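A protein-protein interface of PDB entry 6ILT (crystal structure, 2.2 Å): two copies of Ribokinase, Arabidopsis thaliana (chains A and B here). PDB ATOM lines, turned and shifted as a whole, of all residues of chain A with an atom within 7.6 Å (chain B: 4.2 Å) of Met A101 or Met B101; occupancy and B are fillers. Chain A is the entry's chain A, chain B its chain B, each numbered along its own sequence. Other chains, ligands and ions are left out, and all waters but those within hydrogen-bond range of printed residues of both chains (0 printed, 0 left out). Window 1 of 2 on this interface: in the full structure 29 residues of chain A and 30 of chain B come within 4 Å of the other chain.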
ATOM      1  N   ILE A  15      10.284  -9.886 -16.061  1.00  0.00           N
ATOM      2  CA  ILE A  15      10.437 -10.472 -14.740  1.00  0.00           C
ATOM      3  C   ILE A  15      10.320 -11.996 -14.835  1.00  0.00           C
ATOM      4  O   ILE A  15       9.211 -12.531 -14.868  1.00  0.00           O
ATOM      5  CB  ILE A  15       9.378  -9.922 -13.762  1.00  0.00           C
ATOM      6  CG1 ILE A  15       9.456  -8.398 -13.717  1.00  0.00           C
ATOM      7  CG2 ILE A  15       9.590 -10.500 -12.377  1.00  0.00           C
ATOM      8  CD1 ILE A  15       8.145  -7.729 -13.382  1.00  0.00           C
ATOM      9  N   TYR A  16      11.455 -12.694 -14.915  1.00  0.00           N
ATOM     10  CA  TYR A  16      11.408 -14.153 -15.017  1.00  0.00           C
ATOM     11  C   TYR A  16      11.391 -14.796 -13.642  1.00  0.00           C
ATOM     12  O   TYR A  16      12.166 -14.417 -12.765  1.00  0.00           O
ATOM     13  CB  TYR A  16      12.598 -14.699 -15.792  1.00  0.00           C
ATOM     14  CG  TYR A  16      12.725 -14.222 -17.216  1.00  0.00           C
ATOM     15  CD1 TYR A  16      12.246 -14.989 -18.274  1.00  0.00           C
ATOM     16  CD2 TYR A  16      13.366 -13.027 -17.507  1.00  0.00           C
ATOM     17  CE1 TYR A  16      12.385 -14.566 -19.583  1.00  0.00           C
ATOM     18  CE2 TYR A  16      13.511 -12.597 -18.808  1.00  0.00           C
ATOM     19  CZ  TYR A  16      13.021 -13.367 -19.841  1.00  0.00           C
ATOM     20  OH  TYR A  16      13.165 -12.915 -21.133  1.00  0.00           O
ATOM     21  N   VAL A  17      10.511 -15.771 -13.459  1.00  0.00           N
ATOM     22  CA  VAL A  17      10.513 -16.570 -12.245  1.00  0.00           C
ATOM     23  C   VAL A  17      10.460 -18.077 -12.559  1.00  0.00           C
ATOM     24  O   VAL A  17       9.568 -18.554 -13.269  1.00  0.00           O
ATOM     25  CB  VAL A  17       9.340 -16.180 -11.318  1.00  0.00           C
ATOM     26  CG1 VAL A  17       9.533 -14.762 -10.802  1.00  0.00           C
ATOM     27  CG2 VAL A  17       7.990 -16.319 -12.030  1.00  0.00           C
ATOM     28  N   GLU A  18      11.426 -18.829 -12.040  1.00  0.00           N
ATOM     29  CA  GLU A  18      11.386 -20.274 -12.204  1.00  0.00           C
ATOM     30  C   GLU A  18      10.472 -20.904 -11.171  1.00  0.00           C
ATOM     31  O   GLU A  18      10.733 -20.852  -9.977  1.00  0.00           O
ATOM     32  CB  GLU A  18      12.781 -20.888 -12.124  1.00  0.00           C
ATOM     33  CG  GLU A  18      13.899 -19.968 -12.544  1.00  0.00           C
ATOM     34  CD  GLU A  18      15.159 -20.740 -12.875  1.00  0.00           C
ATOM     35  OE1 GLU A  18      16.132 -20.673 -12.103  1.00  0.00           O
ATOM     36  OE2 GLU A  18      15.166 -21.434 -13.924  1.00  0.00           O
ATOM     37  N   ILE A  19       9.399 -21.512 -11.658  1.00  0.00           N
ATOM     38  CA  ILE A  19       8.350 -22.067 -10.816  1.00  0.00           C
ATOM     39  C   ILE A  19       8.156 -23.560 -11.113  1.00  0.00           C
ATOM     40  O   ILE A  19       8.307 -23.989 -12.257  1.00  0.00           O
ATOM     41  CB  ILE A  19       7.031 -21.302 -11.043  1.00  0.00           C
ATOM     42  CG1 ILE A  19       7.120 -19.912 -10.438  1.00  0.00           C
ATOM     43  CG2 ILE A  19       5.890 -22.002 -10.396  1.00  0.00           C
ATOM     44  CD1 ILE A  19       7.225 -19.939  -8.949  1.00  0.00           C
ATOM     45  N   ARG A  21       5.188 -25.228 -10.505  1.00  0.00           N
ATOM     46  CA  ARG A  21       3.852 -25.178 -11.089  1.00  0.00           C
ATOM     47  C   ARG A  21       3.160 -23.848 -10.775  1.00  0.00           C
ATOM     48  O   ARG A  21       3.283 -23.330  -9.665  1.00  0.00           O
ATOM     49  CB  ARG A  21       2.997 -26.331 -10.564  1.00  0.00           C
ATOM     50  CG  ARG A  21       2.813 -26.304  -9.049  1.00  0.00           C
ATOM     51  CD  ARG A  21       1.421 -26.743  -8.633  1.00  0.00           C
ATOM     52  NE  ARG A  21       1.256 -26.698  -7.183  1.00  0.00           N
ATOM     53  CZ  ARG A  21       0.497 -25.816  -6.537  1.00  0.00           C
ATOM     54  NH1 ARG A  21       0.411 -25.858  -5.215  1.00  0.00           N
ATOM     55  NH2 ARG A  21      -0.179 -24.896  -7.209  1.00  0.00           N
ATOM     56  N   LEU A  22       2.438 -23.301 -11.752  1.00  0.00           N
ATOM     57  CA  LEU A  22       1.640 -22.091 -11.549  1.00  0.00           C
ATOM     58  C   LEU A  22       0.809 -22.244 -10.282  1.00  0.00           C
ATOM     59  O   LEU A  22       0.292 -23.324 -10.018  1.00  0.00           O
ATOM     60  CB  LEU A  22       0.731 -21.837 -12.756  1.00  0.00           C
ATOM     61  CG  LEU A  22       1.372 -21.826 -14.148  1.00  0.00           C
ATOM     62  CD1 LEU A  22       0.293 -21.800 -15.215  1.00  0.00           C
ATOM     63  CD2 LEU A  22       2.333 -20.654 -14.336  1.00  0.00           C
ATOM     64  N   PRO A  23       0.692 -21.180  -9.477  1.00  0.00           N
ATOM     65  CA  PRO A  23      -0.066 -21.338  -8.228  1.00  0.00           C
ATOM     66  C   PRO A  23      -1.565 -21.476  -8.486  1.00  0.00           C
ATOM     67  O   PRO A  23      -2.051 -21.044  -9.534  1.00  0.00           O
ATOM     68  CB  PRO A  23       0.241 -20.048  -7.467  1.00  0.00           C
ATOM     69  CG  PRO A  23       0.454 -19.039  -8.542  1.00  0.00           C
ATOM     70  CD  PRO A  23       1.123 -19.788  -9.690  1.00  0.00           C
ATOM     71  N   GLY A  26      -5.795 -18.235  -5.037  1.00  0.00           N
ATOM     72  CA  GLY A  26      -5.755 -18.168  -3.585  1.00  0.00           C
ATOM     73  C   GLY A  26      -4.391 -18.519  -3.000  1.00  0.00           C
ATOM     74  O   GLY A  26      -4.027 -18.043  -1.921  1.00  0.00           O
ATOM     75  N   ILE A  29       3.008 -19.331  -3.646  1.00  0.00           N
ATOM     76  CA  ILE A  29       4.107 -20.265  -3.890  1.00  0.00           C
ATOM     77  C   ILE A  29       5.453 -19.551  -3.992  1.00  0.00           C
ATOM     78  O   ILE A  29       5.516 -18.331  -4.150  1.00  0.00           O
ATOM     79  CB  ILE A  29       3.892 -21.074  -5.181  1.00  0.00           C
ATOM     80  CG1 ILE A  29       4.048 -20.174  -6.408  1.00  0.00           C
ATOM     81  CG2 ILE A  29       2.527 -21.732  -5.182  1.00  0.00           C
ATOM     82  CD1 ILE A  29       3.907 -20.913  -7.701  1.00  0.00           C
ATOM     83  N   ALA A  98       6.526  -7.541 -17.976  1.00  0.00           N
ATOM     84  CA  ALA A  98       5.963  -8.845 -18.245  1.00  0.00           C
ATOM     85  C   ALA A  98       6.406  -9.842 -17.180  1.00  0.00           C
ATOM     86  O   ALA A  98       7.594  -9.955 -16.858  1.00  0.00           O
ATOM     87  CB  ALA A  98       6.386  -9.321 -19.626  1.00  0.00           C
ATOM     88  N   VAL A  99       5.450 -10.571 -16.631  1.00  0.00           N
ATOM     89  CA  VAL A  99       5.780 -11.635 -15.702  1.00  0.00           C
ATOM     90  C   VAL A  99       5.907 -12.926 -16.497  1.00  0.00           C
ATOM     91  O   VAL A  99       4.918 -13.456 -17.003  1.00  0.00           O
ATOM     92  CB  VAL A  99       4.727 -11.778 -14.598  1.00  0.00           C
ATOM     93  CG1 VAL A  99       5.027 -12.998 -13.737  1.00  0.00           C
ATOM     94  CG2 VAL A  99       4.683 -10.520 -13.742  1.00  0.00           C
ATOM     95  N   VAL A 100       7.136 -13.407 -16.635  1.00  0.00           N
ATOM     96  CA  VAL A 100       7.399 -14.652 -17.350  1.00  0.00           C
ATOM     97  C   VAL A 100       7.563 -15.803 -16.363  1.00  0.00           C
ATOM     98  O   VAL A 100       8.577 -15.909 -15.671  1.00  0.00           O
ATOM     99  CB  VAL A 100       8.656 -14.546 -18.231  1.00  0.00           C
ATOM    100  CG1 VAL A 100       9.039 -15.905 -18.763  1.00  0.00           C
ATOM    101  CG2 VAL A 100       8.411 -13.587 -19.382  1.00  0.00           C
ATOM    102  N   MET A 101       6.543 -16.654 -16.299  1.00  0.00           N
ATOM    103  CA  MET A 101       6.551 -17.827 -15.433  1.00  0.00           C
ATOM    104  C   MET A 101       7.014 -19.096 -16.160  1.00  0.00           C
ATOM    105  O   MET A 101       6.257 -19.742 -16.886  1.00  0.00           O
ATOM    106  CB  MET A 101       5.169 -18.034 -14.835  1.00  0.00           C
ATOM    107  CG  MET A 101       4.862 -17.038 -13.739  1.00  0.00           C
ATOM    108  SD  MET A 101       3.111 -16.686 -13.615  1.00  0.00           S
ATOM    109  CE  MET A 101       2.798 -16.109 -15.285  1.00  0.00           C
ATOM    110  N   LEU A 102       8.279 -19.428 -15.946  1.00  0.00           N
ATOM    111  CA  LEU A 102       8.897 -20.628 -16.481  1.00  0.00           C
ATOM    112  C   LEU A 102       8.608 -21.862 -15.617  1.00  0.00           C
ATOM    113  O   LEU A 102       9.391 -22.194 -14.732  1.00  0.00           O
ATOM    114  CB  LEU A 102      10.400 -20.402 -16.590  1.00  0.00           C
ATOM    115  CG  LEU A 102      10.741 -19.142 -17.381  1.00  0.00           C
ATOM    116  CD1 LEU A 102      12.209 -18.772 -17.212  1.00  0.00           C
ATOM    117  CD2 LEU A 102      10.394 -19.339 -18.855  1.00  0.00           C
ATOM    118  N   GLN A 103       7.485 -22.532 -15.882  1.00  0.00           N
ATOM    119  CA  GLN A 103       7.062 -23.699 -15.104  1.00  0.00           C
ATOM    120  C   GLN A 103       8.032 -24.874 -15.266  1.00  0.00           C
ATOM    121  O   GLN A 103       8.671 -25.025 -16.312  1.00  0.00           O
ATOM    122  CB  GLN A 103       5.647 -24.127 -15.503  1.00  0.00           C
ATOM    123  N   SER A 104       8.138 -25.703 -14.227  1.00  0.00           N
ATOM    124  CA  SER A 104       9.077 -26.826 -14.235  1.00  0.00           C
ATOM    125  C   SER A 104       8.643 -27.902 -15.221  1.00  0.00           C
ATOM    126  O   SER A 104       9.473 -28.648 -15.742  1.00  0.00           O
ATOM    127  CB  SER A 104       9.226 -27.430 -12.835  1.00  0.00           C
ATOM    128  N   GLY A 106       8.161 -27.790 -18.070  1.00  0.00           N
ATOM    129  CA  GLY A 106       8.598 -27.414 -19.401  1.00  0.00           C
ATOM    130  C   GLY A 106       7.778 -26.266 -19.958  1.00  0.00           C
ATOM    131  O   GLY A 106       8.216 -25.557 -20.867  1.00  0.00           O
ATOM    132  N   GLN A 107       6.586 -26.075 -19.401  1.00  0.00           N
ATOM    133  CA  GLN A 107       5.673 -25.048 -19.885  1.00  0.00           C
ATOM    134  C   GLN A 107       6.091 -23.642 -19.450  1.00  0.00           C
ATOM    135  O   GLN A 107       6.877 -23.467 -18.518  1.00  0.00           O
ATOM    136  CB  GLN A 107       4.248 -25.338 -19.407  1.00  0.00           C
ATOM    137  CG  GLN A 107       3.626 -26.597 -20.002  1.00  0.00           C
ATOM    138  CD  GLN A 107       3.031 -26.368 -21.382  1.00  0.00           C
ATOM    139  OE1 GLN A 107       3.653 -25.755 -22.248  1.00  0.00           O
ATOM    140  NE2 GLN A 107       1.813 -26.855 -21.588  1.00  0.00           N
ATOM    141  N   ASN A 108       5.552 -22.645 -20.144  1.00  0.00           N
ATOM    142  CA  ASN A 108       5.822 -21.246 -19.842  1.00  0.00           C
ATOM    143  C   ASN A 108       4.547 -20.410 -19.968  1.00  0.00           C
ATOM    144  O   ASN A 108       3.854 -20.487 -20.980  1.00  0.00           O
ATOM    145  CB  ASN A 108       6.914 -20.702 -20.769  1.00  0.00           C
ATOM    146  N   SER A 109       4.237 -19.620 -18.940  1.00  0.00           N
ATOM    147  CA  SER A 109       3.068 -18.735 -18.968  1.00  0.00           C
ATOM    148  C   SER A 109       3.457 -17.270 -18.723  1.00  0.00           C
ATOM    149  O   SER A 109       4.378 -16.982 -17.960  1.00  0.00           O
ATOM    150  CB  SER A 109       2.044 -19.196 -17.942  1.00  0.00           C
ATOM    151  OG  SER A 109       1.715 -20.551 -18.180  1.00  0.00           O
ATOM    152  N   ILE A 110       2.757 -16.345 -19.375  1.00  0.00           N
ATOM    153  CA  ILE A 110       3.181 -14.944 -19.392  1.00  0.00           C
ATOM    154  C   ILE A 110       2.035 -13.967 -19.102  1.00  0.00           C
ATOM    155  O   ILE A 110       0.915 -14.171 -19.553  1.00  0.00           O
ATOM    156  CB  ILE A 110       3.829 -14.604 -20.748  1.00  0.00           C
ATOM    157  CG1 ILE A 110       5.184 -15.299 -20.852  1.00  0.00           C
ATOM    158  CG2 ILE A 110       4.060 -13.123 -20.885  1.00  0.00           C
ATOM    159  CD1 ILE A 110       5.493 -15.852 -22.195  1.00  0.00           C
ATOM    160  N   ILE A 111       2.312 -12.939 -18.300  1.00  0.00           N
ATOM    161  CA  ILE A 111       1.367 -11.846 -18.085  1.00  0.00           C
ATOM    162  C   ILE A 111       2.018 -10.550 -18.528  1.00  0.00           C
ATOM    163  O   ILE A 111       3.148 -10.242 -18.151  1.00  0.00           O
ATOM    164  CB  ILE A 111       0.927 -11.689 -16.618  1.00  0.00           C
ATOM    165  CG1 ILE A 111       0.300 -12.961 -16.069  1.00  0.00           C
ATOM    166  CG2 ILE A 111      -0.073 -10.553 -16.484  1.00  0.00           C
ATOM    167  CD1 ILE A 111      -0.081 -12.816 -14.598  1.00  0.00           C
ATOM    168  N   VAL B  17       0.090  -7.068 -10.211  1.00  0.00           N
ATOM    169  CA  VAL B  17      -0.552  -6.977 -11.522  1.00  0.00           C
ATOM    170  C   VAL B  17      -2.048  -7.314 -11.420  1.00  0.00           C
ATOM    171  O   VAL B  17      -2.438  -8.239 -10.710  1.00  0.00           O
ATOM    172  CB  VAL B  17       0.140  -7.899 -12.550  1.00  0.00           C
ATOM    173  CG1 VAL B  17       1.639  -7.646 -12.534  1.00  0.00           C
ATOM    174  CG2 VAL B  17      -0.134  -9.377 -12.258  1.00  0.00           C
ATOM    175  N   ILE B  19      -5.201  -8.790 -13.142  1.00  0.00           N
ATOM    176  CA  ILE B  19      -5.645  -9.679 -14.212  1.00  0.00           C
ATOM    177  C   ILE B  19      -7.080 -10.157 -13.979  1.00  0.00           C
ATOM    178  O   ILE B  19      -7.560 -10.166 -12.844  1.00  0.00           O
ATOM    179  CB  ILE B  19      -4.737 -10.909 -14.325  1.00  0.00           C
ATOM    180  CG1 ILE B  19      -4.811 -11.717 -13.027  1.00  0.00           C
ATOM    181  CG2 ILE B  19      -3.309 -10.488 -14.634  1.00  0.00           C
ATOM    182  CD1 ILE B  19      -3.775 -12.798 -12.912  1.00  0.00           C
ATOM    183  N   VAL B  99       5.587 -11.453  -6.821  1.00  0.00           N
ATOM    184  CA  VAL B  99       4.602 -11.138  -7.831  1.00  0.00           C
ATOM    185  C   VAL B  99       3.209 -11.368  -7.258  1.00  0.00           C
ATOM    186  O   VAL B  99       2.804 -12.506  -7.000  1.00  0.00           O
ATOM    187  CB  VAL B  99       4.818 -11.980  -9.093  1.00  0.00           C
ATOM    188  CG1 VAL B  99       3.729 -11.707 -10.101  1.00  0.00           C
ATOM    189  CG2 VAL B  99       6.178 -11.666  -9.681  1.00  0.00           C
ATOM    190  N   VAL B 100       2.490 -10.275  -7.025  1.00  0.00           N
ATOM    191  CA  VAL B 100       1.118 -10.355  -6.539  1.00  0.00           C
ATOM    192  C   VAL B 100       0.094 -10.189  -7.667  1.00  0.00           C
ATOM    193  O   VAL B 100      -0.031  -9.116  -8.264  1.00  0.00           O
ATOM    194  CB  VAL B 100       0.844  -9.306  -5.466  1.00  0.00           C
ATOM    195  CG1 VAL B 100      -0.547  -9.499  -4.920  1.00  0.00           C
ATOM    196  CG2 VAL B 100       1.881  -9.403  -4.343  1.00  0.00           C
ATOM    197  N   MET B 101      -0.635 -11.269  -7.944  1.00  0.00           N
ATOM    198  CA  MET B 101      -1.682 -11.294  -8.964  1.00  0.00           C
ATOM    199  C   MET B 101      -3.092 -11.079  -8.417  1.00  0.00           C
ATOM    200  O   MET B 101      -3.751 -12.028  -7.976  1.00  0.00           O
ATOM    201  CB  MET B 101      -1.627 -12.619  -9.700  1.00  0.00           C
ATOM    202  CG  MET B 101      -0.249 -12.889 -10.209  1.00  0.00           C
ATOM    203  SD  MET B 101      -0.119 -14.441 -11.050  1.00  0.00           S
ATOM    204  CE  MET B 101       1.607 -14.384 -11.515  1.00  0.00           C
ATOM    205  N   LEU B 102      -3.549  -9.831  -8.467  1.00  0.00           N
ATOM    206  CA  LEU B 102      -4.894  -9.478  -8.038  1.00  0.00           C
ATOM    207  C   LEU B 102      -5.932  -9.857  -9.103  1.00  0.00           C
ATOM    208  O   LEU B 102      -6.069  -9.161 -10.109  1.00  0.00           O
ATOM    209  CB  LEU B 102      -4.962  -7.980  -7.726  1.00  0.00           C
ATOM    210  CG  LEU B 102      -3.853  -7.516  -6.785  1.00  0.00           C
ATOM    211  CD1 LEU B 102      -3.946  -6.035  -6.465  1.00  0.00           C
ATOM    212  CD2 LEU B 102      -3.897  -8.333  -5.508  1.00  0.00           C
ATOM    213  N   GLN B 103      -6.659 -10.955  -8.883  1.00  0.00           N
ATOM    214  CA  GLN B 103      -7.668 -11.425  -9.842  1.00  0.00           C
ATOM    215  C   GLN B 103      -8.987 -10.668  -9.757  1.00  0.00           C
ATOM    216  O   GLN B 103      -9.337 -10.120  -8.712  1.00  0.00           O
ATOM    217  CB  GLN B 103      -7.965 -12.905  -9.638  1.00  0.00           C
ATOM    218  CG  GLN B 103      -7.140 -13.847 -10.460  1.00  0.00           C
ATOM    219  CD  GLN B 103      -6.996 -15.176  -9.767  1.00  0.00           C
ATOM    220  OE1 GLN B 103      -7.488 -16.199 -10.246  1.00  0.00           O
ATOM    221  NE2 GLN B 103      -6.315 -15.172  -8.624  1.00  0.00           N
ATOM    222  N   GLN B 107      -9.923 -13.369  -5.747  1.00  0.00           N
ATOM    223  CA  GLN B 107      -8.840 -14.293  -5.415  1.00  0.00           C
ATOM    224  C   GLN B 107      -7.466 -13.672  -5.706  1.00  0.00           C
ATOM    225  O   GLN B 107      -7.289 -12.962  -6.701  1.00  0.00           O
ATOM    226  CB  GLN B 107      -9.004 -15.607  -6.190  1.00  0.00           C
ATOM    227  N   ASN B 108      -6.505 -13.926  -4.820  1.00  0.00           N
ATOM    228  CA  ASN B 108      -5.135 -13.454  -5.000  1.00  0.00           C
ATOM    229  C   ASN B 108      -4.186 -14.620  -5.131  1.00  0.00           C
ATOM    230  O   ASN B 108      -4.384 -15.644  -4.503  1.00  0.00           O
ATOM    231  CB  ASN B 108      -4.690 -12.580  -3.830  1.00  0.00           C
ATOM    232  CG  ASN B 108      -5.619 -11.410  -3.588  1.00  0.00           C
ATOM    233  OD1 ASN B 108      -6.628 -11.249  -4.278  1.00  0.00           O
ATOM    234  ND2 ASN B 108      -5.288 -10.586  -2.600  1.00  0.00           N
ATOM    235  N   SER B 109      -3.148 -14.462  -5.935  1.00  0.00           N
ATOM    236  CA  SER B 109      -2.102 -15.473  -6.021  1.00  0.00           C
ATOM    237  C   SER B 109      -0.735 -14.806  -5.942  1.00  0.00           C
ATOM    238  O   SER B 109      -0.520 -13.735  -6.510  1.00  0.00           O
ATOM    239  CB  SER B 109      -2.237 -16.289  -7.301  1.00  0.00           C
ATOM    240  OG  SER B 109      -3.402 -17.090  -7.257  1.00  0.00           O
ATOM    241  N   ILE B 111       3.661 -15.165  -5.924  1.00  0.00           N
ATOM    242  CA  ILE B 111       4.904 -15.883  -6.189  1.00  0.00           C
ATOM    243  C   ILE B 111       6.047 -15.128  -5.539  1.00  0.00           C
ATOM    244  O   ILE B 111       6.230 -13.942  -5.795  1.00  0.00           O
ATOM    245  CB  ILE B 111       5.175 -16.027  -7.671  1.00  0.00           C
ATOM    246  CG1 ILE B 111       4.069 -16.838  -8.346  1.00  0.00           C
ATOM    247  CG2 ILE B 111       6.545 -16.646  -7.903  1.00  0.00           C
ATOM    248  CD1 ILE B 111       4.207 -16.855  -9.840  1.00  0.00           C
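Hydrophobic or aromatic side chains of chain A that line the printed part of chain B: Ile A19, Ile A29, Val A99, Met A101 and Ile A111.
Printed residues of chain B that touch a printed residue of chain A: Ile B19, Val B99, Met B101, Asn B108, Ser B109 and Ile B111.
Among the printed residues, 9 pairs touch across the chains.
The backbone carbonyl oxygen (O) of Ile A111 is in hydrogen-bond range of the backbone NH (N) of Val A99, 2.8 Å away.
The backbone NH (N) of Met B101 is in hydrogen-bond range of the backbone carbonyl oxygen (O) of Ser B109 (2.9 Å).
The backbone carbonyl oxygen (O) of Leu B102 is in hydrogen-bond range of the backbone NH (N) of Ile B19.
The backbone carbonyl oxygen (O) of Ile A19 is in hydrogen-bond range of the backbone NH (N) of Ser A104 (2.6 Å).
N of Val B99 sits at hydrogen-bond distance from O of Ile B111 (2.8 Å).
O of Leu A102 lies within hydrogen-bond range of N of Ile A19, at 3.1 Å.
Of the printed residues of chain B, Gly A26 touches Asn B108 (3.0 Å) and Ser B109 (3.5 Å).
Printed residues of chain B within 4 Å of Ile A29: Ile B111 (3.2 Å).
Of chain B, only Met B101 (3.5 Å) and Ile B111 (3.9 Å) come within 4 Å of Met A101.
Ser A109 touches none of the printed residues of chain B.
Of the printed residues of chain B, Ile A111 touches Ile B19 and Met B101.
Val B100 touches none of the printed residues of chain A.
Met B101 touches just these residues of chain A: Met A101 and Ile A111.
Of the printed residues of chain A, Ser B109 touches Gly A26 (3.5 Å).
The nearest residue of chain A that does not touch Met B101 is Val A99 (4.3 Å).
O of Asn B108 sits at hydrogen-bond distance from N of Gly A26.
The backbone NH (N) of Gly A26 is in hydrogen-bond range of the side-chain hydroxyl (OG) of Ser B109, at 3.5 Å.
Ile A19 touches Ile B111, and with the chains exchanged Ile A111 touches Ile B19.
Val A99 touches its own counterpart, Val B99.
Met B101 touches its own counterpart, Met A101.
Met A101 touches Ile B111, and with the chains exchanged Ile A111 touches Met B101.
Positions printed for both chains: 17, 19, 99, 100, 101, 102, 103, 107, 108, 109 and 111.
Of the 9 pairs that touch across the chains among the printed residues, 6 have their exchanged pair printed and touching as well.
Ile A19 touches Ile B111 (CD1 to CG2, 3.5 Å).
O of Ile A29 touches CA of Ile B111 (3.2 Å).
CG2 of Val A99 touches CG1 of Val B99, 3.9 Å away.
Met A101 touches Met B101 (SD to CE, 3.5 Å).
Ile B111 touches Met A101.
CG2 of Ile A111 touches CG2 of Ile B19 (3.7 Å).
Met B101 touches Ile A111.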
